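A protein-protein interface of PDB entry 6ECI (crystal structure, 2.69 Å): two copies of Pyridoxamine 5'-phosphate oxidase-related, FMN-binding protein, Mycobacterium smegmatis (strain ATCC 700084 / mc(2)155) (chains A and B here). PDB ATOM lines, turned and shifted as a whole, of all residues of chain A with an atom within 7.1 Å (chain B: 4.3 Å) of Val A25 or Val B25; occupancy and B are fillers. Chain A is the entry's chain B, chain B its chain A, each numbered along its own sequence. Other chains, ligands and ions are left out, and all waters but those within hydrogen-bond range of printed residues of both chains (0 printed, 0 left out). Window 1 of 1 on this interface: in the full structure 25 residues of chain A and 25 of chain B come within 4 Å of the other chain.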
ATOM      1  N   ARG A  23       7.506   5.908 -21.988  1.00  0.00           N
ATOM      2  CA  ARG A  23       8.523   6.167 -20.977  1.00  0.00           C
ATOM      3  C   ARG A  23       9.845   6.532 -21.632  1.00  0.00           C
ATOM      4  O   ARG A  23      10.328   5.810 -22.510  1.00  0.00           O
ATOM      5  CB  ARG A  23       8.704   4.947 -20.071  1.00  0.00           C
ATOM      6  CG  ARG A  23       7.486   4.642 -19.216  1.00  0.00           C
ATOM      7  CD  ARG A  23       7.195   3.159 -19.167  1.00  0.00           C
ATOM      8  NE  ARG A  23       6.595   2.653 -20.395  1.00  0.00           N
ATOM      9  CZ  ARG A  23       5.286   2.553 -20.605  1.00  0.00           C
ATOM     10  NH1 ARG A  23       4.425   2.935 -19.671  1.00  0.00           N
ATOM     11  NH2 ARG A  23       4.837   2.069 -21.754  1.00  0.00           N
ATOM     12  N   ILE A  24      10.421   7.654 -21.201  1.00  0.00           N
ATOM     13  CA  ILE A  24      11.776   8.040 -21.574  1.00  0.00           C
ATOM     14  C   ILE A  24      12.744   7.410 -20.582  1.00  0.00           C
ATOM     15  O   ILE A  24      12.541   7.496 -19.363  1.00  0.00           O
ATOM     16  CB  ILE A  24      11.928   9.570 -21.591  1.00  0.00           C
ATOM     17  CG1 ILE A  24      11.138  10.186 -22.745  1.00  0.00           C
ATOM     18  CG2 ILE A  24      13.395   9.963 -21.692  1.00  0.00           C
ATOM     19  CD1 ILE A  24      11.841  10.123 -24.081  1.00  0.00           C
ATOM     20  N   VAL A  25      13.791   6.770 -21.092  1.00  0.00           N
ATOM     21  CA  VAL A  25      14.822   6.158 -20.260  1.00  0.00           C
ATOM     22  C   VAL A  25      16.142   6.848 -20.571  1.00  0.00           C
ATOM     23  O   VAL A  25      16.604   6.829 -21.719  1.00  0.00           O
ATOM     24  CB  VAL A  25      14.922   4.640 -20.490  1.00  0.00           C
ATOM     25  CG1 VAL A  25      16.095   4.055 -19.718  1.00  0.00           C
ATOM     26  CG2 VAL A  25      13.625   3.957 -20.085  1.00  0.00           C
ATOM     27  N   THR A  26      16.741   7.463 -19.555  1.00  0.00           N
ATOM     28  CA  THR A  26      18.007   8.166 -19.693  1.00  0.00           C
ATOM     29  C   THR A  26      19.074   7.472 -18.860  1.00  0.00           C
ATOM     30  O   THR A  26      18.780   6.859 -17.829  1.00  0.00           O
ATOM     31  CB  THR A  26      17.880   9.634 -19.267  1.00  0.00           C
ATOM     32  OG1 THR A  26      17.362   9.706 -17.932  1.00  0.00           O
ATOM     33  CG2 THR A  26      16.949  10.379 -20.209  1.00  0.00           C
ATOM     34  N   THR A  27      20.322   7.578 -19.310  1.00  0.00           N
ATOM     35  CA  THR A  27      21.425   6.820 -18.733  1.00  0.00           C
ATOM     36  C   THR A  27      22.634   7.716 -18.518  1.00  0.00           C
ATOM     37  O   THR A  27      23.050   8.433 -19.434  1.00  0.00           O
ATOM     38  CB  THR A  27      21.803   5.643 -19.634  1.00  0.00           C
ATOM     39  OG1 THR A  27      20.641   4.844 -19.883  1.00  0.00           O
ATOM     40  CG2 THR A  27      22.871   4.792 -18.975  1.00  0.00           C
ATOM     41  N   SER A  32      20.490   4.402 -14.499  1.00  0.00           N
ATOM     42  CA  SER A  32      19.425   4.854 -15.377  1.00  0.00           C
ATOM     43  C   SER A  32      18.350   5.586 -14.589  1.00  0.00           C
ATOM     44  O   SER A  32      18.195   5.410 -13.379  1.00  0.00           O
ATOM     45  CB  SER A  32      18.804   3.672 -16.123  1.00  0.00           C
ATOM     46  OG  SER A  32      19.732   3.095 -17.024  1.00  0.00           O
ATOM     47  N   HIS A  33      17.610   6.429 -15.302  1.00  0.00           N
ATOM     48  CA  HIS A  33      16.367   7.001 -14.815  1.00  0.00           C
ATOM     49  C   HIS A  33      15.298   6.777 -15.874  1.00  0.00           C
ATOM     50  O   HIS A  33      15.601   6.658 -17.064  1.00  0.00           O
ATOM     51  CB  HIS A  33      16.508   8.496 -14.504  1.00  0.00           C
ATOM     52  CG  HIS A  33      17.200   8.782 -13.208  1.00  0.00           C
ATOM     53  ND1 HIS A  33      18.574   8.802 -13.086  1.00  0.00           N
ATOM     54  CD2 HIS A  33      16.708   9.055 -11.976  1.00  0.00           C
ATOM     55  CE1 HIS A  33      18.898   9.077 -11.835  1.00  0.00           C
ATOM     56  NE2 HIS A  33      17.785   9.234 -11.141  1.00  0.00           N
ATOM     57  N   ILE A  34      14.046   6.698 -15.437  1.00  0.00           N
ATOM     58  CA  ILE A  34      12.928   6.485 -16.345  1.00  0.00           C
ATOM     59  C   ILE A  34      11.863   7.536 -16.068  1.00  0.00           C
ATOM     60  O   ILE A  34      11.578   7.858 -14.909  1.00  0.00           O
ATOM     61  CB  ILE A  34      12.361   5.052 -16.227  1.00  0.00           C
ATOM     62  CG1 ILE A  34      11.190   4.854 -17.191  1.00  0.00           C
ATOM     63  CG2 ILE A  34      11.966   4.740 -14.801  1.00  0.00           C
ATOM     64  CD1 ILE A  34      10.797   3.406 -17.383  1.00  0.00           C
ATOM     65  N   PHE A  35      11.293   8.087 -17.138  1.00  0.00           N
ATOM     66  CA  PHE A  35      10.321   9.175 -17.052  1.00  0.00           C
ATOM     67  C   PHE A  35       9.090   8.830 -17.878  1.00  0.00           C
ATOM     68  O   PHE A  35       9.135   8.894 -19.120  1.00  0.00           O
ATOM     69  CB  PHE A  35      10.928  10.487 -17.536  1.00  0.00           C
ATOM     70  CG  PHE A  35      12.216  10.851 -16.860  1.00  0.00           C
ATOM     71  CD1 PHE A  35      13.425  10.364 -17.330  1.00  0.00           C
ATOM     72  CD2 PHE A  35      12.220  11.695 -15.761  1.00  0.00           C
ATOM     73  CE1 PHE A  35      14.612  10.703 -16.707  1.00  0.00           C
ATOM     74  CE2 PHE A  35      13.405  12.038 -15.138  1.00  0.00           C
ATOM     75  CZ  PHE A  35      14.601  11.542 -15.611  1.00  0.00           C
ATOM     76  N   LEU A  56      13.511  15.795 -15.987  1.00  0.00           N
ATOM     77  CA  LEU A  56      13.414  15.264 -17.345  1.00  0.00           C
ATOM     78  C   LEU A  56      14.100  16.188 -18.343  1.00  0.00           C
ATOM     79  O   LEU A  56      14.751  15.725 -19.287  1.00  0.00           O
ATOM     80  CB  LEU A  56      11.945  15.062 -17.721  1.00  0.00           C
ATOM     81  CG  LEU A  56      11.584  14.712 -19.173  1.00  0.00           C
ATOM     82  CD1 LEU A  56      12.246  13.419 -19.630  1.00  0.00           C
ATOM     83  CD2 LEU A  56      10.071  14.635 -19.340  1.00  0.00           C
ATOM     84  N   ALA A  59      17.861  15.732 -18.010  1.00  0.00           N
ATOM     85  CA  ALA A  59      18.316  14.364 -18.230  1.00  0.00           C
ATOM     86  C   ALA A  59      18.180  13.912 -19.680  1.00  0.00           C
ATOM     87  O   ALA A  59      19.049  13.192 -20.184  1.00  0.00           O
ATOM     88  CB  ALA A  59      17.551  13.400 -17.319  1.00  0.00           C
ATOM     89  N   ALA A  60      17.111  14.312 -20.366  1.00  0.00           N
ATOM     90  CA  ALA A  60      16.799  13.768 -21.682  1.00  0.00           C
ATOM     91  C   ALA A  60      17.188  14.687 -22.829  1.00  0.00           C
ATOM     92  O   ALA A  60      17.729  14.216 -23.834  1.00  0.00           O
ATOM     93  CB  ALA A  60      15.304  13.451 -21.781  1.00  0.00           C
ATOM     94  N   ASN A  64      21.235  11.137 -25.591  1.00  0.00           N
ATOM     95  CA  ASN A  64      20.701   9.899 -26.139  1.00  0.00           C
ATOM     96  C   ASN A  64      19.728   9.285 -25.145  1.00  0.00           C
ATOM     97  O   ASN A  64      20.060   9.100 -23.970  1.00  0.00           O
ATOM     98  CB  ASN A  64      21.833   8.924 -26.451  1.00  0.00           C
ATOM     99  CG  ASN A  64      22.852   9.505 -27.411  1.00  0.00           C
ATOM    100  OD1 ASN A  64      22.502  10.222 -28.349  1.00  0.00           O
ATOM    101  ND2 ASN A  64      24.123   9.209 -27.173  1.00  0.00           N
ATOM    102  N   VAL A  65      18.517   8.978 -25.611  1.00  0.00           N
ATOM    103  CA  VAL A  65      17.463   8.471 -24.747  1.00  0.00           C
ATOM    104  C   VAL A  65      16.849   7.222 -25.362  1.00  0.00           C
ATOM    105  O   VAL A  65      16.909   6.994 -26.572  1.00  0.00           O
ATOM    106  CB  VAL A  65      16.358   9.519 -24.490  1.00  0.00           C
ATOM    107  CG1 VAL A  65      16.940  10.779 -23.865  1.00  0.00           C
ATOM    108  CG2 VAL A  65      15.608   9.834 -25.782  1.00  0.00           C
ATOM    109  N   LEU A  66      16.254   6.411 -24.494  1.00  0.00           N
ATOM    110  CA  LEU A  66      15.371   5.328 -24.895  1.00  0.00           C
ATOM    111  C   LEU A  66      13.925   5.776 -24.743  1.00  0.00           C
ATOM    112  O   LEU A  66      13.574   6.451 -23.771  1.00  0.00           O
ATOM    113  CB  LEU A  66      15.614   4.078 -24.049  1.00  0.00           C
ATOM    114  CG  LEU A  66      16.815   3.215 -24.420  1.00  0.00           C
ATOM    115  CD1 LEU A  66      16.993   2.095 -23.417  1.00  0.00           C
ATOM    116  CD2 LEU A  66      16.600   2.653 -25.799  1.00  0.00           C
ATOM    117  N   PHE A  67      13.091   5.415 -25.711  1.00  0.00           N
ATOM    118  CA  PHE A  67      11.650   5.578 -25.588  1.00  0.00           C
ATOM    119  C   PHE A  67      10.984   4.225 -25.765  1.00  0.00           C
ATOM    120  O   PHE A  67      11.300   3.490 -26.706  1.00  0.00           O
ATOM    121  CB  PHE A  67      11.085   6.559 -26.610  1.00  0.00           C
ATOM    122  CG  PHE A  67       9.587   6.651 -26.577  1.00  0.00           C
ATOM    123  CD1 PHE A  67       8.952   7.430 -25.626  1.00  0.00           C
ATOM    124  CD2 PHE A  67       8.813   5.944 -27.482  1.00  0.00           C
ATOM    125  CE1 PHE A  67       7.577   7.515 -25.585  1.00  0.00           C
ATOM    126  CE2 PHE A  67       7.436   6.023 -27.445  1.00  0.00           C
ATOM    127  CZ  PHE A  67       6.816   6.810 -26.493  1.00  0.00           C
ATOM    128  N   GLU A  68      10.056   3.906 -24.872  1.00  0.00           N
ATOM    129  CA  GLU A  68       9.355   2.637 -24.942  1.00  0.00           C
ATOM    130  C   GLU A  68       7.878   2.855 -24.655  1.00  0.00           C
ATOM    131  O   GLU A  68       7.496   3.741 -23.888  1.00  0.00           O
ATOM    132  CB  GLU A  68       9.944   1.615 -23.961  1.00  0.00           C
ATOM    133  CG  GLU A  68       9.461   0.198 -24.182  1.00  0.00           C
ATOM    134  CD  GLU A  68       8.255  -0.146 -23.335  1.00  0.00           C
ATOM    135  OE1 GLU A  68       7.897   0.664 -22.454  1.00  0.00           O
ATOM    136  OE2 GLU A  68       7.669  -1.229 -23.548  1.00  0.00           O
ATOM    137  N   ARG B  23       8.201  -2.906 -16.960  1.00  0.00           N
ATOM    138  CA  ARG B  23       9.464  -2.958 -17.688  1.00  0.00           C
ATOM    139  C   ARG B  23      10.639  -3.069 -16.728  1.00  0.00           C
ATOM    140  O   ARG B  23      10.728  -2.313 -15.753  1.00  0.00           O
ATOM    141  CB  ARG B  23       9.644  -1.724 -18.578  1.00  0.00           C
ATOM    142  CG  ARG B  23       8.559  -1.539 -19.623  1.00  0.00           C
ATOM    143  CD  ARG B  23       7.453  -0.622 -19.122  1.00  0.00           C
ATOM    144  NE  ARG B  23       6.177  -0.904 -19.775  1.00  0.00           N
ATOM    145  CZ  ARG B  23       4.992  -0.611 -19.251  1.00  0.00           C
ATOM    146  NH1 ARG B  23       3.878  -0.906 -19.907  1.00  0.00           N
ATOM    147  NH2 ARG B  23       4.919  -0.022 -18.066  1.00  0.00           N
ATOM    148  N   ILE B  24      11.533  -4.015 -17.008  1.00  0.00           N
ATOM    149  CA  ILE B  24      12.845  -4.093 -16.381  1.00  0.00           C
ATOM    150  C   ILE B  24      13.794  -3.210 -17.178  1.00  0.00           C
ATOM    151  O   ILE B  24      13.758  -3.207 -18.412  1.00  0.00           O
ATOM    152  CB  ILE B  24      13.346  -5.549 -16.337  1.00  0.00           C
ATOM    153  CG1 ILE B  24      12.453  -6.402 -15.435  1.00  0.00           C
ATOM    154  CG2 ILE B  24      14.798  -5.612 -15.879  1.00  0.00           C
ATOM    155  CD1 ILE B  24      12.548  -6.052 -13.966  1.00  0.00           C
ATOM    156  N   VAL B  25      14.638  -2.448 -16.483  1.00  0.00           N
ATOM    157  CA  VAL B  25      15.638  -1.603 -17.127  1.00  0.00           C
ATOM    158  C   VAL B  25      16.998  -1.932 -16.523  1.00  0.00           C
ATOM    159  O   VAL B  25      17.230  -1.686 -15.331  1.00  0.00           O
ATOM    160  CB  VAL B  25      15.323  -0.107 -16.987  1.00  0.00           C
ATOM    161  CG1 VAL B  25      16.424   0.726 -17.627  1.00  0.00           C
ATOM    162  CG2 VAL B  25      13.988   0.213 -17.628  1.00  0.00           C
ATOM    163  N   THR B  26      17.893  -2.482 -17.339  1.00  0.00           N
ATOM    164  CA  THR B  26      19.259  -2.801 -16.947  1.00  0.00           C
ATOM    165  C   THR B  26      20.219  -1.760 -17.510  1.00  0.00           C
ATOM    166  O   THR B  26      19.918  -1.076 -18.488  1.00  0.00           O
ATOM    167  CB  THR B  26      19.645  -4.198 -17.440  1.00  0.00           C
ATOM    168  OG1 THR B  26      19.532  -4.246 -18.868  1.00  0.00           O
ATOM    169  CG2 THR B  26      18.728  -5.253 -16.830  1.00  0.00           C
ATOM    170  N   SER B  32      21.941   1.318 -21.670  1.00  0.00           N
ATOM    171  CA  SER B  32      20.860   0.713 -20.909  1.00  0.00           C
ATOM    172  C   SER B  32      19.894  -0.011 -21.837  1.00  0.00           C
ATOM    173  O   SER B  32      19.757   0.333 -23.014  1.00  0.00           O
ATOM    174  CB  SER B  32      20.102   1.759 -20.092  1.00  0.00           C
ATOM    175  OG  SER B  32      19.177   2.460 -20.902  1.00  0.00           O
ATOM    176  N   HIS B  33      19.224  -1.020 -21.286  1.00  0.00           N
ATOM    177  CA  HIS B  33      18.245  -1.815 -22.007  1.00  0.00           C
ATOM    178  C   HIS B  33      16.960  -1.893 -21.196  1.00  0.00           C
ATOM    179  O   HIS B  33      16.983  -1.835 -19.964  1.00  0.00           O
ATOM    180  CB  HIS B  33      18.768  -3.225 -22.288  1.00  0.00           C
ATOM    181  CG  HIS B  33      19.862  -3.266 -23.305  1.00  0.00           C
ATOM    182  ND1 HIS B  33      21.165  -2.929 -23.010  1.00  0.00           N
ATOM    183  CD2 HIS B  33      19.845  -3.595 -24.619  1.00  0.00           C
ATOM    184  CE1 HIS B  33      21.906  -3.054 -24.097  1.00  0.00           C
ATOM    185  NE2 HIS B  33      21.129  -3.456 -25.087  1.00  0.00           N
ATOM    186  N   ILE B  34      15.838  -2.028 -21.895  1.00  0.00           N
ATOM    187  CA  ILE B  34      14.530  -2.090 -21.260  1.00  0.00           C
ATOM    188  C   ILE B  34      13.816  -3.348 -21.737  1.00  0.00           C
ATOM    189  O   ILE B  34      13.837  -3.672 -22.929  1.00  0.00           O
ATOM    190  CB  ILE B  34      13.701  -0.815 -21.542  1.00  0.00           C
ATOM    191  CG1 ILE B  34      12.260  -0.982 -21.063  1.00  0.00           C
ATOM    192  CG2 ILE B  34      13.756  -0.438 -23.011  1.00  0.00           C
ATOM    193  CD1 ILE B  34      11.512   0.326 -20.953  1.00  0.00           C
ATOM    194  N   VAL B  65      18.774  -3.507 -11.004  1.00  0.00           N
ATOM    195  CA  VAL B  65      17.808  -3.287 -12.069  1.00  0.00           C
ATOM    196  C   VAL B  65      16.843  -2.187 -11.647  1.00  0.00           C
ATOM    197  O   VAL B  65      16.804  -1.759 -10.493  1.00  0.00           O
ATOM    198  CB  VAL B  65      17.023  -4.566 -12.433  1.00  0.00           C
ATOM    199  CG1 VAL B  65      17.965  -5.708 -12.770  1.00  0.00           C
ATOM    200  CG2 VAL B  65      16.084  -4.952 -11.302  1.00  0.00           C
ATOM    201  N   LEU B  66      16.061  -1.733 -12.619  1.00  0.00           N
ATOM    202  CA  LEU B  66      14.943  -0.830 -12.410  1.00  0.00           C
ATOM    203  C   LEU B  66      13.672  -1.536 -12.846  1.00  0.00           C
ATOM    204  O   LEU B  66      13.656  -2.209 -13.879  1.00  0.00           O
ATOM    205  CB  LEU B  66      15.106   0.463 -13.217  1.00  0.00           C
ATOM    206  CG  LEU B  66      15.884   1.625 -12.608  1.00  0.00           C
ATOM    207  CD1 LEU B  66      16.044   2.739 -13.627  1.00  0.00           C
ATOM    208  CD2 LEU B  66      15.169   2.132 -11.386  1.00  0.00           C
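The side-chain hydroxyl (OG) of Ser B32 sits at hydrogen-bond distance from the side-chain hydroxyl (OG1) of Thr A27. The guanidinium group of Arg B23 sits close to the guanidinium group of Arg A23. The side-chain carboxylate of Glu A68 is in salt-bridge range of the guanidinium group of Arg B23 (3.5 Å).
The backbone NH of Val B25 sits at hydrogen-bond distance from the backbone carbonyl oxygen of Leu B66, at 2.8 Å. The guanidinium group of Arg A23 is in salt-bridge range of the side-chain carboxylate of Glu A68. The backbone carbonyl oxygen of Leu A66 lies within hydrogen-bond range of the backbone NH of Val A25 (2.7 Å). The side-chain hydroxyl (OG) of Ser A32 lies within hydrogen-bond range of the side-chain hydroxyl (OG1) of Thr A27, 3.5 Å away.
Val A25 touches Val B25. CG1 of Val A25 touches OG of Ser B32, at 3.7 Å. CB of Ser B32 touches OG of Ser A32 (3.4 Å). Ser A32 touches Leu B66 (O to CD1, 3.4 Å). O of Ser B32 touches CD1 of Leu A66, 3.3 Å away. Glu A68 touches Ile B34 (CB to CD1, 3.6 Å).
Val A25 touches two residues of chain B. Val B25 touches just one residue of chain A: Val A25. Printed residues of chain A within 4 Å of Arg B23: Arg A23 (3.4 Å) and Glu A68 (3.5 Å). Of the printed residues of chain B, Arg A23 touches Arg B23 (3.4 Å). Printed residues of chain B within 4 Å of Glu A68: Arg B23 (3.5 Å) and Ile B34 (3.6 Å). Thr B26 touches none of the printed residues of chain A.
Of the 9 printed residues of chain B, 5 touch a printed residue of chain A. Hydrophobic or aromatic side chains of chain B within 4 Å of the printed part of chain A: Val B25, Ile B34 and Leu B66. Among the printed residues, Asp or Glu carboxylates within 4 Å of a Lys or Arg side-chain nitrogen of the other chain: Glu A68 with Arg B23.
Arg B23 touches its own counterpart, Arg A23. Val A25 touches its own counterpart, Val B25. Val A25 touches Ser B32, but with the chains exchanged Ser A32 does not touch Val B25 (4.1 Å). Ser A32 touches its own counterpart, Ser B32.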
